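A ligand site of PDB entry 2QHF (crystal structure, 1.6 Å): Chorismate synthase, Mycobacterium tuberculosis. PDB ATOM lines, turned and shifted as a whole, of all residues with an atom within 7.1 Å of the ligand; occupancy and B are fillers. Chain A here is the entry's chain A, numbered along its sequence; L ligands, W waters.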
ATOM      1  N   ARG A  40       3.700  -6.723 -11.276  1.00  0.00           N
ATOM      2  CA  ARG A  40       3.448  -6.321 -12.691  1.00  0.00           C
ATOM      3  C   ARG A  40       2.252  -5.402 -12.896  1.00  0.00           C
ATOM      4  O   ARG A  40       2.085  -4.848 -13.977  1.00  0.00           O
ATOM      5  CB  ARG A  40       3.228  -7.561 -13.566  1.00  0.00           C
ATOM      6  CG  ARG A  40       4.384  -8.517 -13.569  1.00  0.00           C
ATOM      7  CD  ARG A  40       4.057  -9.713 -14.513  1.00  0.00           C
ATOM      8  NE  ARG A  40       3.998  -9.346 -15.920  1.00  0.00           N
ATOM      9  CZ  ARG A  40       2.889  -9.239 -16.672  1.00  0.00           C
ATOM     10  NH1 ARG A  40       1.684  -9.511 -16.198  1.00  0.00           N
ATOM     11  NH2 ARG A  40       2.996  -8.868 -17.935  1.00  0.00           N
ATOM     12  N   ARG A  46      -1.284   1.676 -15.618  1.00  0.00           N
ATOM     13  CA  ARG A  46      -1.149   0.237 -15.869  1.00  0.00           C
ATOM     14  C   ARG A  46      -2.509  -0.450 -16.050  1.00  0.00           C
ATOM     15  O   ARG A  46      -2.613  -1.476 -16.748  1.00  0.00           O
ATOM     16  CB  ARG A  46      -0.376  -0.420 -14.711  1.00  0.00           C
ATOM     17  CG  ARG A  46      -0.032  -1.894 -14.939  1.00  0.00           C
ATOM     18  CD  ARG A  46       0.798  -2.120 -16.186  1.00  0.00           C
ATOM     19  NE  ARG A  46       1.217  -3.519 -16.226  1.00  0.00           N
ATOM     20  CZ  ARG A  46       1.807  -4.113 -17.264  1.00  0.00           C
ATOM     21  NH1 ARG A  46       2.063  -3.448 -18.379  1.00  0.00           N
ATOM     22  NH2 ARG A  46       2.109  -5.402 -17.156  1.00  0.00           N
ATOM     23  N   ARG A  49      -3.892  -1.552 -19.337  1.00  0.00           N
ATOM     24  CA  ARG A  49      -3.333  -2.773 -19.937  1.00  0.00           C
ATOM     25  C   ARG A  49      -3.800  -4.047 -19.231  1.00  0.00           C
ATOM     26  O   ARG A  49      -4.058  -5.060 -19.887  1.00  0.00           O
ATOM     27  CB  ARG A  49      -1.803  -2.707 -19.883  1.00  0.00           C
ATOM     28  CG  ARG A  49      -1.105  -3.964 -20.352  1.00  0.00           C
ATOM     29  CD  ARG A  49      -1.468  -4.331 -21.780  1.00  0.00           C
ATOM     30  NE  ARG A  49      -0.672  -5.471 -22.215  1.00  0.00           N
ATOM     31  CZ  ARG A  49      -0.899  -6.227 -23.287  1.00  0.00           C
ATOM     32  NH1 ARG A  49      -1.950  -5.990 -24.066  1.00  0.00           N
ATOM     33  NH2 ARG A  49      -0.093  -7.249 -23.575  1.00  0.00           N
ATOM     34  N   MET A  50      -3.868  -3.999 -17.908  1.00  0.00           N
ATOM     35  CA  MET A  50      -4.240  -5.166 -17.115  1.00  0.00           C
ATOM     36  C   MET A  50      -5.662  -5.055 -16.578  1.00  0.00           C
ATOM     37  O   MET A  50      -6.064  -3.994 -16.099  1.00  0.00           O
ATOM     38  CB  MET A  50      -3.246  -5.368 -15.978  1.00  0.00           C
ATOM     39  CG  MET A  50      -1.863  -5.788 -16.488  1.00  0.00           C
ATOM     40  SD  MET A  50      -0.760  -6.266 -15.173  1.00  0.00           S
ATOM     41  CE  MET A  50      -1.353  -7.912 -14.729  1.00  0.00           C
ATOM     42  N   ALA A 138       3.727  -9.274 -24.581  1.00  0.00           N
ATOM     43  CA  ALA A 138       4.355  -9.181 -23.260  1.00  0.00           C
ATOM     44  C   ALA A 138       3.560  -9.795 -22.119  1.00  0.00           C
ATOM     45  O   ALA A 138       4.037  -9.916 -20.985  1.00  0.00           O
ATOM     46  CB  ALA A 138       4.739  -7.745 -22.941  1.00  0.00           C
ATOM     47  N   ARG A 139       2.340 -10.284 -22.395  1.00  0.00           N
ATOM     48  CA  ARG A 139       1.631 -11.107 -21.426  1.00  0.00           C
ATOM     49  C   ARG A 139       2.496 -12.323 -21.000  1.00  0.00           C
ATOM     50  O   ARG A 139       2.416 -12.772 -19.875  1.00  0.00           O
ATOM     51  CB  ARG A 139       0.287 -11.557 -22.007  1.00  0.00           C
ATOM     52  CG  ARG A 139      -0.412 -12.628 -21.186  1.00  0.00           C
ATOM     53  CD  ARG A 139      -0.705 -12.146 -19.797  1.00  0.00           C
ATOM     54  NE  ARG A 139      -1.563 -13.091 -19.076  1.00  0.00           N
ATOM     55  CZ  ARG A 139      -1.759 -13.081 -17.753  1.00  0.00           C
ATOM     56  NH1 ARG A 139      -1.154 -12.177 -16.974  1.00  0.00           N
ATOM     57  NH2 ARG A 139      -2.557 -13.984 -17.200  1.00  0.00           N
ATOM     58  N   THR A 141       5.491 -12.361 -20.261  1.00  0.00           N
ATOM     59  CA  THR A 141       6.364 -11.990 -19.132  1.00  0.00           C
ATOM     60  C   THR A 141       5.810 -12.333 -17.760  1.00  0.00           C
ATOM     61  O   THR A 141       6.543 -12.437 -16.775  1.00  0.00           O
ATOM     62  CB  THR A 141       6.848 -10.519 -19.174  1.00  0.00           C
ATOM     63  OG1 THR A 141       5.752  -9.631 -18.865  1.00  0.00           O
ATOM     64  CG2 THR A 141       7.473 -10.158 -20.527  1.00  0.00           C
ATOM     65  N   ALA A 142       4.481 -12.546 -17.654  1.00  0.00           N
ATOM     66  CA  ALA A 142       3.912 -13.086 -16.440  1.00  0.00           C
ATOM     67  C   ALA A 142       4.494 -14.466 -16.091  1.00  0.00           C
ATOM     68  O   ALA A 142       4.804 -14.753 -14.947  1.00  0.00           O
ATOM     69  CB  ALA A 142       2.388 -13.181 -16.571  1.00  0.00           C
ATOM     70  N   ILE A 255      13.943  -9.735 -23.422  1.00  0.00           N
ATOM     71  CA  ILE A 255      12.646  -9.225 -22.971  1.00  0.00           C
ATOM     72  C   ILE A 255      12.042  -8.371 -24.076  1.00  0.00           C
ATOM     73  O   ILE A 255      12.705  -7.573 -24.744  1.00  0.00           O
ATOM     74  CB  ILE A 255      12.790  -8.411 -21.679  1.00  0.00           C
ATOM     75  CG1 ILE A 255      13.305  -9.283 -20.524  1.00  0.00           C
ATOM     76  CG2 ILE A 255      11.455  -7.749 -21.285  1.00  0.00           C
ATOM     77  CD1 ILE A 255      13.868  -8.475 -19.395  1.00  0.00           C
ATOM     78  N   GLN A 256      10.744  -8.540 -24.285  1.00  0.00           N
ATOM     79  CA  GLN A 256      10.010  -7.726 -25.241  1.00  0.00           C
ATOM     80  C   GLN A 256      10.309  -6.225 -25.082  1.00  0.00           C
ATOM     81  O   GLN A 256      10.379  -5.737 -23.964  1.00  0.00           O
ATOM     82  CB  GLN A 256       8.507  -7.948 -25.023  1.00  0.00           C
ATOM     83  CG  GLN A 256       7.957  -9.359 -25.433  1.00  0.00           C
ATOM     84  CD  GLN A 256       8.103 -10.452 -24.390  1.00  0.00           C
ATOM     85  OE1 GLN A 256       9.002 -10.436 -23.543  1.00  0.00           O
ATOM     86  NE2 GLN A 256       7.196 -11.432 -24.436  1.00  0.00           N
ATOM     87  N   ALA A 257      10.514  -5.579 -26.223  1.00  0.00           N
ATOM     88  CA  ALA A 257      10.693  -4.120 -26.352  1.00  0.00           C
ATOM     89  C   ALA A 257      12.041  -3.587 -25.886  1.00  0.00           C
ATOM     90  O   ALA A 257      12.272  -2.380 -25.976  1.00  0.00           O
ATOM     91  CB  ALA A 257       9.558  -3.368 -25.653  1.00  0.00           C
ATOM     92  N   ILE A 258      12.930  -4.455 -25.406  1.00  0.00           N
ATOM     93  CA  ILE A 258      14.251  -3.991 -24.955  1.00  0.00           C
ATOM     94  C   ILE A 258      15.181  -3.859 -26.174  1.00  0.00           C
ATOM     95  O   ILE A 258      15.266  -4.766 -27.007  1.00  0.00           O
ATOM     96  CB  ILE A 258      14.840  -4.924 -23.889  1.00  0.00           C
ATOM     97  CG1 ILE A 258      13.933  -5.026 -22.666  1.00  0.00           C
ATOM     98  CG2 ILE A 258      16.248  -4.441 -23.466  1.00  0.00           C
ATOM     99  CD1 ILE A 258      13.487  -3.707 -22.080  1.00  0.00           C
ATOM    100  N   MET A 314      14.065   0.449 -22.994  1.00  0.00           N
ATOM    101  CA  MET A 314      12.789  -0.054 -23.526  1.00  0.00           C
ATOM    102  C   MET A 314      12.224   0.936 -24.524  1.00  0.00           C
ATOM    103  O   MET A 314      12.080   2.114 -24.192  1.00  0.00           O
ATOM    104  CB  MET A 314      11.807  -0.253 -22.396  1.00  0.00           C
ATOM    105  CG  MET A 314      10.531  -0.918 -22.858  1.00  0.00           C
ATOM    106  SD  MET A 314       9.369  -0.988 -21.485  1.00  0.00           S
ATOM    107  CE  MET A 314       7.983  -1.754 -22.271  1.00  0.00           C
ATOM    108  N   LYS A 315      11.898   0.465 -25.714  1.00  0.00           N
ATOM    109  CA  LYS A 315      11.266   1.307 -26.715  1.00  0.00           C
ATOM    110  C   LYS A 315       9.787   1.421 -26.317  1.00  0.00           C
ATOM    111  O   LYS A 315       9.264   0.609 -25.580  1.00  0.00           O
ATOM    112  CB  LYS A 315      11.390   0.739 -28.101  1.00  0.00           C
ATOM    113  CG  LYS A 315      10.555  -0.508 -28.421  1.00  0.00           C
ATOM    114  CD  LYS A 315      10.913  -1.051 -29.770  1.00  0.00           C
ATOM    115  CE  LYS A 315      10.073  -2.237 -30.171  1.00  0.00           C
ATOM    116  NZ  LYS A 315      10.569  -2.854 -31.452  1.00  0.00           N
ATOM    117  N   ILE A 317       6.038   0.565 -26.528  1.00  0.00           N
ATOM    118  CA  ILE A 317       5.823  -0.876 -26.787  1.00  0.00           C
ATOM    119  C   ILE A 317       4.351  -0.814 -27.333  1.00  0.00           C
ATOM    120  O   ILE A 317       3.927  -1.671 -28.109  1.00  0.00           O
ATOM    121  CB  ILE A 317       5.915  -1.880 -25.598  1.00  0.00           C
ATOM    122  CG1 ILE A 317       5.638  -3.295 -26.131  1.00  0.00           C
ATOM    123  CG2 ILE A 317       4.946  -1.569 -24.481  1.00  0.00           C
ATOM    124  CD1 ILE A 317       5.919  -4.419 -25.157  1.00  0.00           C
ATOM    125  N   ARG A 341      -2.641  -2.609 -27.633  1.00  0.00           N
ATOM    126  CA  ARG A 341      -2.663  -2.154 -26.252  1.00  0.00           C
ATOM    127  C   ARG A 341      -2.754  -0.631 -26.246  1.00  0.00           C
ATOM    128  O   ARG A 341      -2.374   0.028 -27.213  1.00  0.00           O
ATOM    129  CB  ARG A 341      -1.437  -2.654 -25.475  1.00  0.00           C
ATOM    130  CG  ARG A 341      -0.117  -2.460 -26.170  1.00  0.00           C
ATOM    131  CD  ARG A 341       0.998  -3.286 -25.523  1.00  0.00           C
ATOM    132  NE  ARG A 341       1.264  -2.836 -24.165  1.00  0.00           N
ATOM    133  CZ  ARG A 341       2.007  -3.478 -23.282  1.00  0.00           C
ATOM    134  NH1 ARG A 341       2.585  -4.646 -23.581  1.00  0.00           N
ATOM    135  NH2 ARG A 341       2.170  -2.953 -22.078  1.00  0.00           N
ATOM    136  N   ASP A 343      -2.007   1.359 -23.196  1.00  0.00           N
ATOM    137  CA  ASP A 343      -1.264   2.013 -22.121  1.00  0.00           C
ATOM    138  C   ASP A 343      -0.178   2.931 -22.697  1.00  0.00           C
ATOM    139  O   ASP A 343       0.403   2.657 -23.745  1.00  0.00           O
ATOM    140  CB  ASP A 343      -0.667   1.003 -21.155  1.00  0.00           C
ATOM    141  CG  ASP A 343       0.171  -0.043 -21.845  1.00  0.00           C
ATOM    142  OD1 ASP A 343      -0.228  -0.545 -22.937  1.00  0.00           O
ATOM    143  OD2 ASP A 343       1.235  -0.377 -21.274  1.00  0.00           O
ATOM    144  N   ALA A 346       4.893   1.346 -20.218  1.00  0.00           N
ATOM    145  CA  ALA A 346       4.993   0.120 -19.428  1.00  0.00           C
ATOM    146  C   ALA A 346       6.353  -0.042 -18.741  1.00  0.00           C
ATOM    147  O   ALA A 346       6.662  -1.118 -18.249  1.00  0.00           O
ATOM    148  CB  ALA A 346       4.764  -1.070 -20.331  1.00  0.00           C
ATOM    149  N   VAL A 347       7.108   1.040 -18.652  1.00  0.00           N
ATOM    150  CA  VAL A 347       8.466   0.961 -18.099  1.00  0.00           C
ATOM    151  C   VAL A 347       8.538   0.473 -16.647  1.00  0.00           C
ATOM    152  O   VAL A 347       9.343  -0.390 -16.319  1.00  0.00           O
ATOM    153  CB  VAL A 347       9.202   2.310 -18.325  1.00  0.00           C
ATOM    154  CG1 VAL A 347      10.578   2.308 -17.660  1.00  0.00           C
ATOM    155  CG2 VAL A 347       9.374   2.573 -19.791  1.00  0.00           C
ATOM    156  N   ALA A 349       6.549  -1.516 -14.916  1.00  0.00           N
ATOM    157  CA  ALA A 349       6.277  -2.961 -14.903  1.00  0.00           C
ATOM    158  C   ALA A 349       7.393  -3.753 -15.596  1.00  0.00           C
ATOM    159  O   ALA A 349       7.744  -4.859 -15.162  1.00  0.00           O
ATOM    160  CB  ALA A 349       4.956  -3.240 -15.583  1.00  0.00           C
ATOM    161  N   ALA A 350       7.934  -3.205 -16.673  1.00  0.00           N
ATOM    162  CA  ALA A 350       9.072  -3.827 -17.370  1.00  0.00           C
ATOM    163  C   ALA A 350      10.262  -4.009 -16.436  1.00  0.00           C
ATOM    164  O   ALA A 350      10.989  -5.014 -16.517  1.00  0.00           O
ATOM    165  CB  ALA A 350       9.456  -3.033 -18.578  1.00  0.00           C
ATOM    166  N   GLY A 351      10.454  -3.070 -15.505  1.00  0.00           N
ATOM    167  CA  GLY A 351      11.493  -3.211 -14.488  1.00  0.00           C
ATOM    168  C   GLY A 351      11.404  -4.474 -13.666  1.00  0.00           C
ATOM    169  O   GLY A 351      12.416  -5.102 -13.327  1.00  0.00           O
ATOM    170  N   VAL A 353      10.179  -7.220 -14.694  1.00  0.00           N
ATOM    171  CA  VAL A 353      10.549  -8.343 -15.545  1.00  0.00           C
ATOM    172  C   VAL A 353      12.098  -8.395 -15.647  1.00  0.00           C
ATOM    173  O   VAL A 353      12.692  -9.468 -15.622  1.00  0.00           O
ATOM    174  CB  VAL A 353       9.887  -8.234 -16.913  1.00  0.00           C
ATOM    175  CG1 VAL A 353      10.278  -9.417 -17.824  1.00  0.00           C
ATOM    176  CG2 VAL A 353       8.348  -8.224 -16.751  1.00  0.00           C
ATOM    177  N   VAL A 354      12.717  -7.226 -15.743  1.00  0.00           N
ATOM    178  CA  VAL A 354      14.198  -7.197 -15.768  1.00  0.00           C
ATOM    179  C   VAL A 354      14.738  -7.822 -14.488  1.00  0.00           C
ATOM    180  O   VAL A 354      15.704  -8.633 -14.529  1.00  0.00           O
ATOM    181  CB  VAL A 354      14.727  -5.774 -15.984  1.00  0.00           C
ATOM    182  CG1 VAL A 354      16.278  -5.738 -15.959  1.00  0.00           C
ATOM    183  CG2 VAL A 354      14.217  -5.219 -17.297  1.00  0.00           C
HETATM  184  N1  LIG L   1       8.217  -6.177 -20.255  1.00  0.00           N
HETATM  185  C1  LIG L   1       6.971  -6.149 -19.759  1.00  0.00           C
HETATM  186  C2  LIG L   1       5.951  -5.435 -20.431  1.00  0.00           C
HETATM  187  C3  LIG L   1       6.225  -4.799 -21.616  1.00  0.00           C
HETATM  188  C4  LIG L   1       7.537  -4.869 -22.104  1.00  0.00           C
HETATM  189  C5  LIG L   1       8.503  -5.562 -21.403  1.00  0.00           C
HETATM  190  C6  LIG L   1       4.543  -5.444 -19.913  1.00  0.00           C
HETATM  191  O1  LIG L   1       3.638  -4.894 -20.522  1.00  0.00           O
HETATM  192  N2  LIG L   1       4.328  -6.139 -18.833  1.00  0.00           N
HETATM  193  O   HOH W   1       5.429  -6.830 -16.235  1.00  0.00           O
HETATM  194  O   HOH W   2       1.634  -6.740 -21.116  1.00  0.00           O
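The guanidinium group (NH2) of Arg 341 sits at hydrogen-bond distance from an oxygen (O1) of the ligand, 2.9 Å away. O1 of the ligand is in hydrogen-bond range of NH1 of Arg 46 (3.0 Å).
The guanidinium group (NE) of Arg 46 is in hydrogen-bond range of the side-chain sulfur (SD) of Met 50 (3.5 Å). O of Arg 40 lies within hydrogen-bond range of NE of Arg 46, 2.8 Å away. NH2 of Arg 40 sits at hydrogen-bond distance from OG1 of Thr 141 (3.0 Å). OD2 of Asp 343 is in salt-bridge range of NH2 of Arg 341 (2.9 Å). O of Ala 138 sits at hydrogen-bond distance from OG1 of Thr 141 (2.7 Å). NH2 of Arg 40 is in hydrogen-bond range of O of Ala 138 (3.4 Å).
The guanidinium group (NH2) of Arg 40 sits close to a nitrogen (N2) of the ligand (3.2 Å). Merely in contact with the ligand: Met 314 (3.2 Å), Gln 256 (3.2 Å), Ile 317 (3.5 Å), Ala 138 (3.6 Å), Ile 255 (3.7 Å), Thr 141 (3.8 Å), Ala 350 (3.8 Å), Val 353 (3.9 Å) and Ala 346 (3.99 Å). Hydrophobic or aromatic side chains within 4 Å of the ligand: Ala 138, Ile 255, Met 314, Ile 317, Ala 346, Ala 350 and Val 353. Within 4 Å of the ligand: Arg 40, Arg 46, Ala 138, Thr 141, Ile 255, Gln 256, Met 314, Ile 317, Arg 341, Ala 346, Ala 350 and Val 353. The nearest printed residue that does not touch the ligand is Ala 257 (4.4 Å).
Water W2 lies within hydrogen-bond range of O1 of the ligand (2.8 Å), NE of Arg 49 (2.9 Å) and NH1 of Arg 341 (3.4 Å). Water W1 lies within hydrogen-bond range of a nitrogen (N2) of the ligand, the guanidinium group of Arg 40 and the backbone carbonyl oxygen of Ala 349.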
